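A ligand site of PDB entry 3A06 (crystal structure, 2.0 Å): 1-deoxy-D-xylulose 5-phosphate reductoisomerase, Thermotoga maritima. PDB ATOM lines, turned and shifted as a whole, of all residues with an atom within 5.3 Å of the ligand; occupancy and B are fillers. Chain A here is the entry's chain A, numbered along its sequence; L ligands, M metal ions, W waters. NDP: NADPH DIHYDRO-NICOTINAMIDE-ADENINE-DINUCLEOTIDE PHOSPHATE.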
ATOM      1  N   GLY A  10      16.291   2.829  12.219  1.00  0.00           N
ATOM      2  CA  GLY A  10      17.454   3.062  11.407  1.00  0.00           C
ATOM      3  C   GLY A  10      18.722   2.728  12.203  1.00  0.00           C
ATOM      4  O   GLY A  10      19.667   3.504  12.198  1.00  0.00           O
ATOM      5  N   ALA A  11      18.753   1.568  12.880  1.00  0.00           N
ATOM      6  CA  ALA A  11      19.909   1.240  13.744  1.00  0.00           C
ATOM      7  C   ALA A  11      21.216   0.981  13.019  1.00  0.00           C
ATOM      8  O   ALA A  11      22.314   1.054  13.634  1.00  0.00           O
ATOM      9  CB  ALA A  11      19.581   0.084  14.671  1.00  0.00           C
ATOM     10  N   THR A  12      21.114   0.685  11.716  1.00  0.00           N
ATOM     11  CA  THR A  12      22.249   0.248  10.945  1.00  0.00           C
ATOM     12  C   THR A  12      22.939   1.415  10.250  1.00  0.00           C
ATOM     13  O   THR A  12      23.946   1.221   9.592  1.00  0.00           O
ATOM     14  CB  THR A  12      21.831  -0.766   9.882  1.00  0.00           C
ATOM     15  OG1 THR A  12      20.742  -0.223   9.131  1.00  0.00           O
ATOM     16  CG2 THR A  12      21.392  -2.076  10.552  1.00  0.00           C
ATOM     17  N   GLY A  13      22.403   2.623  10.417  1.00  0.00           N
ATOM     18  CA  GLY A  13      22.986   3.786   9.799  1.00  0.00           C
ATOM     19  C   GLY A  13      24.020   4.507  10.656  1.00  0.00           C
ATOM     20  O   GLY A  13      24.404   4.041  11.701  1.00  0.00           O
ATOM     21  N   SER A  14      24.468   5.669  10.173  1.00  0.00           N
ATOM     22  CA  SER A  14      25.497   6.456  10.856  1.00  0.00           C
ATOM     23  C   SER A  14      25.057   6.890  12.252  1.00  0.00           C
ATOM     24  O   SER A  14      25.744   6.599  13.244  1.00  0.00           O
ATOM     25  CB  SER A  14      25.871   7.668  10.011  1.00  0.00           C
ATOM     26  OG  SER A  14      26.766   8.513  10.732  1.00  0.00           O
ATOM     27  N   ILE A  15      23.916   7.551  12.344  1.00  0.00           N
ATOM     28  CA  ILE A  15      23.383   7.966  13.663  1.00  0.00           C
ATOM     29  C   ILE A  15      23.054   6.765  14.531  1.00  0.00           C
ATOM     30  O   ILE A  15      23.370   6.744  15.717  1.00  0.00           O
ATOM     31  CB  ILE A  15      22.179   8.908  13.512  1.00  0.00           C
ATOM     32  CG1 ILE A  15      22.607  10.184  12.767  1.00  0.00           C
ATOM     33  CG2 ILE A  15      21.565   9.263  14.879  1.00  0.00           C
ATOM     34  CD1 ILE A  15      23.707  10.974  13.481  1.00  0.00           C
ATOM     35  N   GLY A  16      22.466   5.739  13.913  1.00  0.00           N
ATOM     36  CA  GLY A  16      22.061   4.535  14.651  1.00  0.00           C
ATOM     37  C   GLY A  16      23.209   3.849  15.351  1.00  0.00           C
ATOM     38  O   GLY A  16      23.123   3.522  16.521  1.00  0.00           O
ATOM     39  N   GLN A  18      26.168   5.135  16.028  1.00  0.00           N
ATOM     40  CA  GLN A  18      26.732   6.054  17.023  1.00  0.00           C
ATOM     41  C   GLN A  18      25.921   6.050  18.321  1.00  0.00           C
ATOM     42  O   GLN A  18      26.484   6.155  19.401  1.00  0.00           O
ATOM     43  CB  GLN A  18      26.851   7.455  16.453  1.00  0.00           C
ATOM     44  CG  GLN A  18      28.015   7.537  15.429  1.00  0.00           C
ATOM     45  CD  GLN A  18      28.149   8.912  14.816  1.00  0.00           C
ATOM     46  OE1 GLN A  18      27.500   9.236  13.818  1.00  0.00           O
ATOM     47  NE2 GLN A  18      28.984   9.725  15.408  1.00  0.00           N
ATOM     48  N   SER A  35      14.908  -0.906  14.051  1.00  0.00           N
ATOM     49  CA  SER A  35      14.394  -1.063  12.697  1.00  0.00           C
ATOM     50  C   SER A  35      15.583  -0.882  11.812  1.00  0.00           C
ATOM     51  O   SER A  35      16.525  -0.149  12.153  1.00  0.00           O
ATOM     52  CB  SER A  35      13.335  -0.014  12.367  1.00  0.00           C
ATOM     53  OG  SER A  35      13.922   1.147  11.780  1.00  0.00           O
ATOM     54  N   PHE A  36      15.573  -1.570  10.674  1.00  0.00           N
ATOM     55  CA  PHE A  36      16.583  -1.327   9.648  1.00  0.00           C
ATOM     56  C   PHE A  36      15.896  -1.597   8.306  1.00  0.00           C
ATOM     57  O   PHE A  36      14.753  -2.063   8.297  1.00  0.00           O
ATOM     58  CB  PHE A  36      17.812  -2.231   9.833  1.00  0.00           C
ATOM     59  CG  PHE A  36      17.544  -3.694   9.576  1.00  0.00           C
ATOM     60  CD1 PHE A  36      16.960  -4.488  10.543  1.00  0.00           C
ATOM     61  CD2 PHE A  36      17.912  -4.270   8.365  1.00  0.00           C
ATOM     62  CE1 PHE A  36      16.724  -5.828  10.288  1.00  0.00           C
ATOM     63  CE2 PHE A  36      17.664  -5.610   8.105  1.00  0.00           C
ATOM     64  CZ  PHE A  36      17.082  -6.383   9.061  1.00  0.00           C
ATOM     65  N   HIS A  37      16.579  -1.278   7.204  1.00  0.00           N
ATOM     66  CA  HIS A  37      15.959  -1.334   5.887  1.00  0.00           C
ATOM     67  C   HIS A  37      16.411  -2.571   5.121  1.00  0.00           C
ATOM     68  O   HIS A  37      15.613  -3.468   4.898  1.00  0.00           O
ATOM     69  CB  HIS A  37      16.261  -0.054   5.116  1.00  0.00           C
ATOM     70  CG  HIS A  37      15.508   0.070   3.821  1.00  0.00           C
ATOM     71  ND1 HIS A  37      14.135   0.166   3.772  1.00  0.00           N
ATOM     72  CD2 HIS A  37      15.938   0.138   2.540  1.00  0.00           C
ATOM     73  CE1 HIS A  37      13.754   0.292   2.501  1.00  0.00           C
ATOM     74  NE2 HIS A  37      14.827   0.262   1.741  1.00  0.00           N
ATOM     75  N   SER A  38      17.697  -2.636   4.778  1.00  0.00           N
ATOM     76  CA  SER A  38      18.232  -3.770   4.043  1.00  0.00           C
ATOM     77  C   SER A  38      19.611  -4.297   4.501  1.00  0.00           C
ATOM     78  O   SER A  38      20.022  -5.377   4.069  1.00  0.00           O
ATOM     79  CB  SER A  38      18.302  -3.414   2.558  1.00  0.00           C
ATOM     80  OG  SER A  38      19.392  -2.530   2.374  1.00  0.00           O
ATOM     81  N   ASN A  39      20.330  -3.567   5.360  1.00  0.00           N
ATOM     82  CA  ASN A  39      21.636  -4.070   5.834  1.00  0.00           C
ATOM     83  C   ASN A  39      21.572  -5.209   6.864  1.00  0.00           C
ATOM     84  O   ASN A  39      21.870  -5.030   8.060  1.00  0.00           O
ATOM     85  CB  ASN A  39      22.576  -2.946   6.302  1.00  0.00           C
ATOM     86  CG  ASN A  39      24.035  -3.398   6.443  1.00  0.00           C
ATOM     87  OD1 ASN A  39      24.315  -4.598   6.553  1.00  0.00           O
ATOM     88  ND2 ASN A  39      24.950  -2.452   6.441  1.00  0.00           N
ATOM     89  N   THR A  58      11.990  -2.937   7.119  1.00  0.00           N
ATOM     90  CA  THR A  58      11.359  -1.859   6.461  1.00  0.00           C
ATOM     91  C   THR A  58      11.599  -2.042   4.946  1.00  0.00           C
ATOM     92  O   THR A  58      10.816  -1.582   4.114  1.00  0.00           O
ATOM     93  CB  THR A  58      11.940  -0.585   7.120  1.00  0.00           C
ATOM     94  OG1 THR A  58      10.902   0.149   7.794  1.00  0.00           O
ATOM     95  CG2 THR A  58      12.723   0.247   6.201  1.00  0.00           C
ATOM     96  N   ILE A  77       7.205  -0.456  11.543  1.00  0.00           N
ATOM     97  CA  ILE A  77       7.669   0.482  12.590  1.00  0.00           C
ATOM     98  C   ILE A  77       6.509   0.827  13.470  1.00  0.00           C
ATOM     99  O   ILE A  77       6.593   0.707  14.689  1.00  0.00           O
ATOM    100  CB  ILE A  77       8.326   1.749  11.986  1.00  0.00           C
ATOM    101  CG1 ILE A  77       9.729   1.398  11.454  1.00  0.00           C
ATOM    102  CG2 ILE A  77       8.415   2.873  13.044  1.00  0.00           C
ATOM    103  CD1 ILE A  77      10.447   2.553  10.700  1.00  0.00           C
ATOM    104  N   ALA A  92      16.233   7.659  13.366  1.00  0.00           N
ATOM    105  CA  ALA A  92      17.452   7.860  12.614  1.00  0.00           C
ATOM    106  C   ALA A  92      17.329   7.186  11.253  1.00  0.00           C
ATOM    107  O   ALA A  92      18.331   6.794  10.652  1.00  0.00           O
ATOM    108  CB  ALA A  92      18.624   7.280  13.387  1.00  0.00           C
ATOM    109  N   VAL A  93      16.117   7.085  10.739  1.00  0.00           N
ATOM    110  CA  VAL A  93      15.930   6.641   9.346  1.00  0.00           C
ATOM    111  C   VAL A  93      16.277   7.771   8.386  1.00  0.00           C
ATOM    112  O   VAL A  93      16.187   8.942   8.717  1.00  0.00           O
ATOM    113  CB  VAL A  93      14.502   6.062   9.059  1.00  0.00           C
ATOM    114  CG1 VAL A  93      14.242   4.828   9.901  1.00  0.00           C
ATOM    115  CG2 VAL A  93      13.442   7.067   9.300  1.00  0.00           C
ATOM    116  N   SER A  94      16.712   7.410   7.177  1.00  0.00           N
ATOM    117  CA  SER A  94      17.053   8.438   6.225  1.00  0.00           C
ATOM    118  C   SER A  94      15.908   8.597   5.254  1.00  0.00           C
ATOM    119  O   SER A  94      15.140   7.661   5.036  1.00  0.00           O
ATOM    120  CB  SER A  94      18.318   8.062   5.435  1.00  0.00           C
ATOM    121  OG  SER A  94      18.068   6.876   4.714  1.00  0.00           O
ATOM    122  N   GLY A  95      15.785   9.799   4.694  1.00  0.00           N
ATOM    123  CA  GLY A  95      14.864  10.024   3.603  1.00  0.00           C
ATOM    124  C   GLY A  95      13.454  10.343   4.047  1.00  0.00           C
ATOM    125  O   GLY A  95      13.192  10.669   5.211  1.00  0.00           O
ATOM    126  N   SER A  97      10.833   8.476   4.319  1.00  0.00           N
ATOM    127  CA  SER A  97      10.245   7.540   5.291  1.00  0.00           C
ATOM    128  C   SER A  97      10.242   8.078   6.730  1.00  0.00           C
ATOM    129  O   SER A  97       9.474   7.625   7.586  1.00  0.00           O
ATOM    130  CB  SER A  97      11.059   6.251   5.326  1.00  0.00           C
ATOM    131  OG  SER A  97      12.370   6.572   5.815  1.00  0.00           O
ATOM    132  N   ALA A 115      16.505  12.636  14.579  1.00  0.00           N
ATOM    133  CA  ALA A 115      17.650  12.873  13.708  1.00  0.00           C
ATOM    134  C   ALA A 115      17.201  13.153  12.246  1.00  0.00           C
ATOM    135  O   ALA A 115      17.779  14.041  11.558  1.00  0.00           O
ATOM    136  CB  ALA A 115      18.635  11.720  13.800  1.00  0.00           C
ATOM    137  N   ASN A 116      16.132  12.501  11.806  1.00  0.00           N
ATOM    138  CA  ASN A 116      15.600  12.676  10.447  1.00  0.00           C
ATOM    139  C   ASN A 116      15.088  14.070  10.141  1.00  0.00           C
ATOM    140  O   ASN A 116      14.160  14.552  10.799  1.00  0.00           O
ATOM    141  CB  ASN A 116      14.483  11.663  10.166  1.00  0.00           C
ATOM    142  CG  ASN A 116      13.956  11.764   8.732  1.00  0.00           C
ATOM    143  OD1 ASN A 116      13.068  12.589   8.447  1.00  0.00           O
ATOM    144  ND2 ASN A 116      14.494  10.929   7.823  1.00  0.00           N
ATOM    145  N   LYS A 117      15.644  14.668   9.098  1.00  0.00           N
ATOM    146  CA  LYS A 117      15.331  16.043   8.713  1.00  0.00           C
ATOM    147  C   LYS A 117      14.094  16.176   7.844  1.00  0.00           C
ATOM    148  O   LYS A 117      13.344  17.165   7.937  1.00  0.00           O
ATOM    149  CB  LYS A 117      16.502  16.628   7.906  1.00  0.00           C
ATOM    150  CG  LYS A 117      17.817  16.673   8.657  1.00  0.00           C
ATOM    151  CD  LYS A 117      18.758  17.708   8.052  1.00  0.00           C
ATOM    152  CE  LYS A 117      20.149  17.479   8.555  1.00  0.00           C
ATOM    153  NZ  LYS A 117      20.208  17.684  10.043  1.00  0.00           N
ATOM    154  N   GLU A 118      13.888  15.198   6.967  1.00  0.00           N
ATOM    155  CA  GLU A 118      12.820  15.283   5.976  1.00  0.00           C
ATOM    156  C   GLU A 118      11.453  15.425   6.623  1.00  0.00           C
ATOM    157  O   GLU A 118      10.575  16.111   6.100  1.00  0.00           O
ATOM    158  CB  GLU A 118      12.884  14.090   5.005  1.00  0.00           C
ATOM    159  CG  GLU A 118      14.100  14.121   4.030  1.00  0.00           C
ATOM    160  CD  GLU A 118      15.476  13.786   4.681  1.00  0.00           C
ATOM    161  OE1 GLU A 118      16.532  14.086   4.051  1.00  0.00           O
ATOM    162  OE2 GLU A 118      15.513  13.228   5.819  1.00  0.00           O
ATOM    163  N   ASP A 142      20.375  16.596  15.699  1.00  0.00           N
ATOM    164  CA  ASP A 142      21.292  17.380  14.854  1.00  0.00           C
ATOM    165  C   ASP A 142      22.157  18.351  15.722  1.00  0.00           C
ATOM    166  O   ASP A 142      21.633  18.975  16.633  1.00  0.00           O
ATOM    167  CB  ASP A 142      20.438  18.098  13.805  1.00  0.00           C
ATOM    168  CG  ASP A 142      21.161  19.169  13.088  1.00  0.00           C
ATOM    169  OD1 ASP A 142      21.699  18.895  11.989  1.00  0.00           O
ATOM    170  OD2 ASP A 142      21.154  20.318  13.600  1.00  0.00           O
ATOM    171  N   SER A 143      23.470  18.420  15.464  1.00  0.00           N
ATOM    172  CA  SER A 143      24.383  19.204  16.317  1.00  0.00           C
ATOM    173  C   SER A 143      23.931  20.644  16.433  1.00  0.00           C
ATOM    174  O   SER A 143      23.974  21.218  17.525  1.00  0.00           O
ATOM    175  CB  SER A 143      25.816  19.209  15.769  1.00  0.00           C
ATOM    176  OG  SER A 143      25.834  19.822  14.506  1.00  0.00           O
ATOM    177  N   ASN A 191      31.848  13.044   9.957  1.00  0.00           N
ATOM    178  CA  ASN A 191      31.839  11.674   9.428  1.00  0.00           C
ATOM    179  C   ASN A 191      30.410  11.172   9.179  1.00  0.00           C
ATOM    180  O   ASN A 191      29.781  10.585  10.058  1.00  0.00           O
ATOM    181  CB  ASN A 191      32.582  10.736  10.386  1.00  0.00           C
ATOM    182  CG  ASN A 191      34.054  10.621  10.069  1.00  0.00           C
ATOM    183  OD1 ASN A 191      34.431  10.059   9.034  1.00  0.00           O
ATOM    184  ND2 ASN A 191      34.891  11.135  10.956  1.00  0.00           N
ATOM    185  N   MET A 192      29.931  11.368   7.952  1.00  0.00           N
ATOM    186  CA  MET A 192      28.520  11.144   7.644  1.00  0.00           C
ATOM    187  C   MET A 192      28.309  10.325   6.364  1.00  0.00           C
ATOM    188  O   MET A 192      29.239  10.148   5.578  1.00  0.00           O
ATOM    189  CB  MET A 192      27.783  12.488   7.505  1.00  0.00           C
ATOM    190  CG  MET A 192      28.297  13.614   8.403  1.00  0.00           C
ATOM    191  SD  MET A 192      27.473  15.184   8.053  1.00  0.00           S
ATOM    192  CE  MET A 192      28.119  15.582   6.424  1.00  0.00           C
ATOM    193  N   GLY A 193      27.076   9.850   6.175  1.00  0.00           N
ATOM    194  CA  GLY A 193      26.668   9.156   4.935  1.00  0.00           C
ATOM    195  C   GLY A 193      26.948   9.930   3.650  1.00  0.00           C
ATOM    196  O   GLY A 193      27.143  11.147   3.682  1.00  0.00           O
ATOM    197  N   ILE A 196      24.645  13.159   2.828  1.00  0.00           N
ATOM    198  CA  ILE A 196      24.774  14.346   3.666  1.00  0.00           C
ATOM    199  C   ILE A 196      26.017  15.080   3.260  1.00  0.00           C
ATOM    200  O   ILE A 196      26.053  16.311   3.250  1.00  0.00           O
ATOM    201  CB  ILE A 196      24.788  14.012   5.189  1.00  0.00           C
ATOM    202  CG1 ILE A 196      23.879  12.822   5.442  1.00  0.00           C
ATOM    203  CG2 ILE A 196      24.315  15.226   5.976  1.00  0.00           C
ATOM    204  CD1 ILE A 196      23.901  12.298   6.848  1.00  0.00           C
ATOM    205  N   ASN A 205      21.852  20.814   2.875  1.00  0.00           N
ATOM    206  CA  ASN A 205      21.687  20.390   4.269  1.00  0.00           C
ATOM    207  C   ASN A 205      21.375  21.541   5.183  1.00  0.00           C
ATOM    208  O   ASN A 205      20.481  21.454   6.026  1.00  0.00           O
ATOM    209  CB  ASN A 205      22.874  19.582   4.796  1.00  0.00           C
ATOM    210  CG  ASN A 205      22.621  19.080   6.197  1.00  0.00           C
ATOM    211  OD1 ASN A 205      21.743  18.240   6.389  1.00  0.00           O
ATOM    212  ND2 ASN A 205      23.339  19.609   7.167  1.00  0.00           N
ATOM    213  N   MET A 254      28.985  13.500  16.797  1.00  0.00           N
ATOM    214  CA  MET A 254      27.529  13.360  16.955  1.00  0.00           C
ATOM    215  C   MET A 254      27.164  12.564  18.203  1.00  0.00           C
ATOM    216  O   MET A 254      26.027  12.618  18.660  1.00  0.00           O
ATOM    217  CB  MET A 254      26.908  12.703  15.702  1.00  0.00           C
ATOM    218  CG  MET A 254      26.851  13.631  14.474  1.00  0.00           C
ATOM    219  SD  MET A 254      25.906  15.138  14.811  1.00  0.00           S
ATOM    220  CE  MET A 254      24.274  14.541  15.210  1.00  0.00           C
HETATM  221  PA  NDP L   1      22.264   6.533   6.864  1.00  0.00           P
HETATM  222  O1A NDP L   1      22.021   6.393   5.406  1.00  0.00           O
HETATM  223  O2A NDP L   1      23.762   6.371   7.374  1.00  0.00           O
HETATM  224  O5B NDP L   1      21.321   5.464   7.614  1.00  0.00           O
HETATM  225  C5B NDP L   1      19.908   5.614   7.611  1.00  0.00           C
HETATM  226  C4B NDP L   1      19.183   4.435   8.300  1.00  0.00           C
HETATM  227  O4B NDP L   1      17.831   4.409   7.749  1.00  0.00           O
HETATM  228  C3B NDP L   1      19.741   3.028   8.020  1.00  0.00           C
HETATM  229  O3B NDP L   1      19.304   2.166   9.065  1.00  0.00           O
HETATM  230  C2B NDP L   1      18.989   2.583   6.779  1.00  0.00           C
HETATM  231  O2B NDP L   1      18.877   1.140   6.747  1.00  0.00           O
HETATM  232  C1B NDP L   1      17.605   3.127   7.100  1.00  0.00           C
HETATM  233  N9A NDP L   1      16.733   3.365   5.906  1.00  0.00           N
HETATM  234  C8A NDP L   1      17.134   3.669   4.666  1.00  0.00           C
HETATM  235  N7A NDP L   1      16.066   3.816   3.869  1.00  0.00           N
HETATM  236  C5A NDP L   1      14.988   3.583   4.627  1.00  0.00           C
HETATM  237  C6A NDP L   1      13.622   3.570   4.365  1.00  0.00           C
HETATM  238  N6A NDP L   1      13.196   3.840   3.126  1.00  0.00           N
HETATM  239  N1A NDP L   1      12.766   3.307   5.379  1.00  0.00           N
HETATM  240  C2A NDP L   1      13.191   3.047   6.618  1.00  0.00           C
HETATM  241  N3A NDP L   1      14.497   3.026   6.886  1.00  0.00           N
HETATM  242  C4A NDP L   1      15.410   3.307   5.923  1.00  0.00           C
HETATM  243  O3  NDP L   1      21.730   7.983   7.337  1.00  0.00           O
HETATM  244  PN  NDP L   1      22.375   8.825   8.566  1.00  0.00           P
HETATM  245  O1N NDP L   1      23.644   9.496   8.199  1.00  0.00           O
HETATM  246  O2N NDP L   1      22.406   7.945   9.912  1.00  0.00           O
HETATM  247  O5D NDP L   1      21.212   9.903   8.819  1.00  0.00           O
HETATM  248  C5D NDP L   1      19.859   9.539   9.180  1.00  0.00           C
HETATM  249  C4D NDP L   1      19.023  10.820   9.324  1.00  0.00           C
HETATM  250  O4D NDP L   1      19.715  11.634  10.348  1.00  0.00           O
HETATM  251  C3D NDP L   1      19.026  11.657   8.037  1.00  0.00           C
HETATM  252  O3D NDP L   1      17.773  12.327   7.862  1.00  0.00           O
HETATM  253  C2D NDP L   1      20.144  12.673   8.274  1.00  0.00           C
HETATM  254  O2D NDP L   1      19.911  13.903   7.569  1.00  0.00           O
HETATM  255  C1D NDP L   1      20.025  12.916   9.775  1.00  0.00           C
HETATM  256  N1N NDP L   1      21.294  13.463  10.299  1.00  0.00           N
HETATM  257  C2N NDP L   1      22.501  12.760  10.149  1.00  0.00           C
HETATM  258  C3N NDP L   1      23.680  13.303  10.650  1.00  0.00           C
HETATM  259  C7N NDP L   1      24.975  12.539  10.462  1.00  0.00           C
HETATM  260  O7N NDP L   1      26.021  13.008  10.904  1.00  0.00           O
HETATM  261  N7N NDP L   1      24.894  11.377   9.814  1.00  0.00           N
HETATM  262  C4N NDP L   1      23.703  14.674  11.386  1.00  0.00           C
HETATM  263  C5N NDP L   1      22.445  15.276  11.500  1.00  0.00           C
HETATM  264  C6N NDP L   1      21.276  14.707  10.969  1.00  0.00           C
HETATM  265  P2B NDP L   1      20.010   0.261   5.961  1.00  0.00           P
HETATM  266  O1X NDP L   1      21.392   0.637   6.338  1.00  0.00           O
HETATM  267  O2X NDP L   1      19.681  -1.235   6.339  1.00  0.00           O
HETATM  268  O3X NDP L   1      19.719   0.516   4.451  1.00  0.00           O
HETATM  269 MG    MG M   1      23.685  19.428  11.339  1.00  0.00          MG
HETATM  270  O   HOH W   1      14.266   1.222   9.094  1.00  0.00           O
HETATM  271  O   HOH W   2      23.678  17.670  10.235  1.00  0.00           O
HETATM  272  O   HOH W   3      21.163   5.843  11.380  1.00  0.00           O
HETATM  273  O   HOH W   4      24.527  17.515  12.883  1.00  0.00           O
HETATM  274  O   HOH W   5      28.151  11.686  11.987  1.00  0.00           O
HETATM  275  O   HOH W   6      23.877   0.194   6.666  1.00  0.00           O
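O of Ala 115 sits close to O4D of the ligand, 3.3 Å away.
Merely in contact with the ligand: Thr 58 (2.9 Å), Ile 196 (3.1 Å), Val 93 (3.3 Å), Asn 116 (3.4 Å), Met 192 (3.4 Å), Ala 92 (3.4 Å), Met 254 (3.7 Å), Asp 142 (3.7 Å) and Ala 11 (3.9 Å).
Of the 32 residues printed, 22 come within 4 Å of the ligand.
The nearest printed residue that does not touch the ligand is Gly 193 (4.0001 Å).
Water W6 lies within hydrogen-bond range of O1X of the ligand, ND2 of Asn 39 and O of Thr 12.
Water W3 lies within hydrogen-bond range of O2N of the ligand, N of Gly 16, O of Gly 10, O of Ala 92 and N of Ile 15.
Water W1 lies within hydrogen-bond range of OG of Ser 35, N3A of the ligand and O of Phe 36.
Water W4 lies within hydrogen-bond range of the backbone NH (N) of Ser 143 (2.9 Å) and the side-chain sulfur (SD) of Met 254 (3.4 Å).
The backbone NH (N) of Ser 94 sits at hydrogen-bond distance from an oxygen (O4B) of the ligand (3.3 Å).
An oxygen (O2A) of the ligand lies within hydrogen-bond range of the backbone NH (N) of Ser 14.
An oxygen (O2X) of the ligand lies within hydrogen-bond range of the backbone NH of Asn 39.
O2X of the ligand sits at hydrogen-bond distance from N of His 37 (3.2 Å).
OE2 of Glu 118 lies within hydrogen-bond range of O3D of the ligand (3.2 Å).
An oxygen (O2N) of the ligand is in hydrogen-bond range of the backbone NH of Ile 15 (2.9 Å).
A nitrogen (N1A) of the ligand is in hydrogen-bond range of the side-chain hydroxyl (OG) of Ser 97 (3.3 Å).
The backbone NH (N) of Gly 13 lies within hydrogen-bond range of an oxygen (O3B) of the ligand (3.4 Å).
The side-chain hydroxyl of Thr 12 sits at hydrogen-bond distance from an oxygen (O3B) of the ligand.
The backbone NH of Lys 117 sits at hydrogen-bond distance from an oxygen (O3D) of the ligand (3.4 Å).
The backbone carbonyl oxygen (O) of Gly 10 sits close to an oxygen (O3B) of the ligand (3.4 Å).
The backbone NH (N) of Ser 38 is in hydrogen-bond range of an oxygen (O2X) of the ligand (2.9 Å).
The backbone NH (N) of Ala 11 sits at hydrogen-bond distance from the backbone carbonyl oxygen (O) of Ser 35 (2.9 Å).
The side-chain amide nitrogen (ND2) of Asn 116 is in hydrogen-bond range of the backbone carbonyl oxygen (O) of Gly 95 (2.9 Å).
The side-chain hydroxyl (OG) of Ser 35 is in hydrogen-bond range of the backbone NH (N) of Gly 10, 2.9 Å away.
The backbone NH of Thr 58 lies within hydrogen-bond range of the backbone carbonyl oxygen of Phe 36 (3.1 Å).
ND2 of Asn 116 lies within hydrogen-bond range of O of Val 93.
The side-chain amide oxygen (OE1) of Gln 18 lies close to the backbone carbonyl oxygen (O) of Ser 14.
The backbone NH of Glu 118 sits at hydrogen-bond distance from the side-chain amide oxygen of Asn 116 (3.1 Å).
NZ of Lys 117 lies close to OD1 of Asp 142 (2.7 Å).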
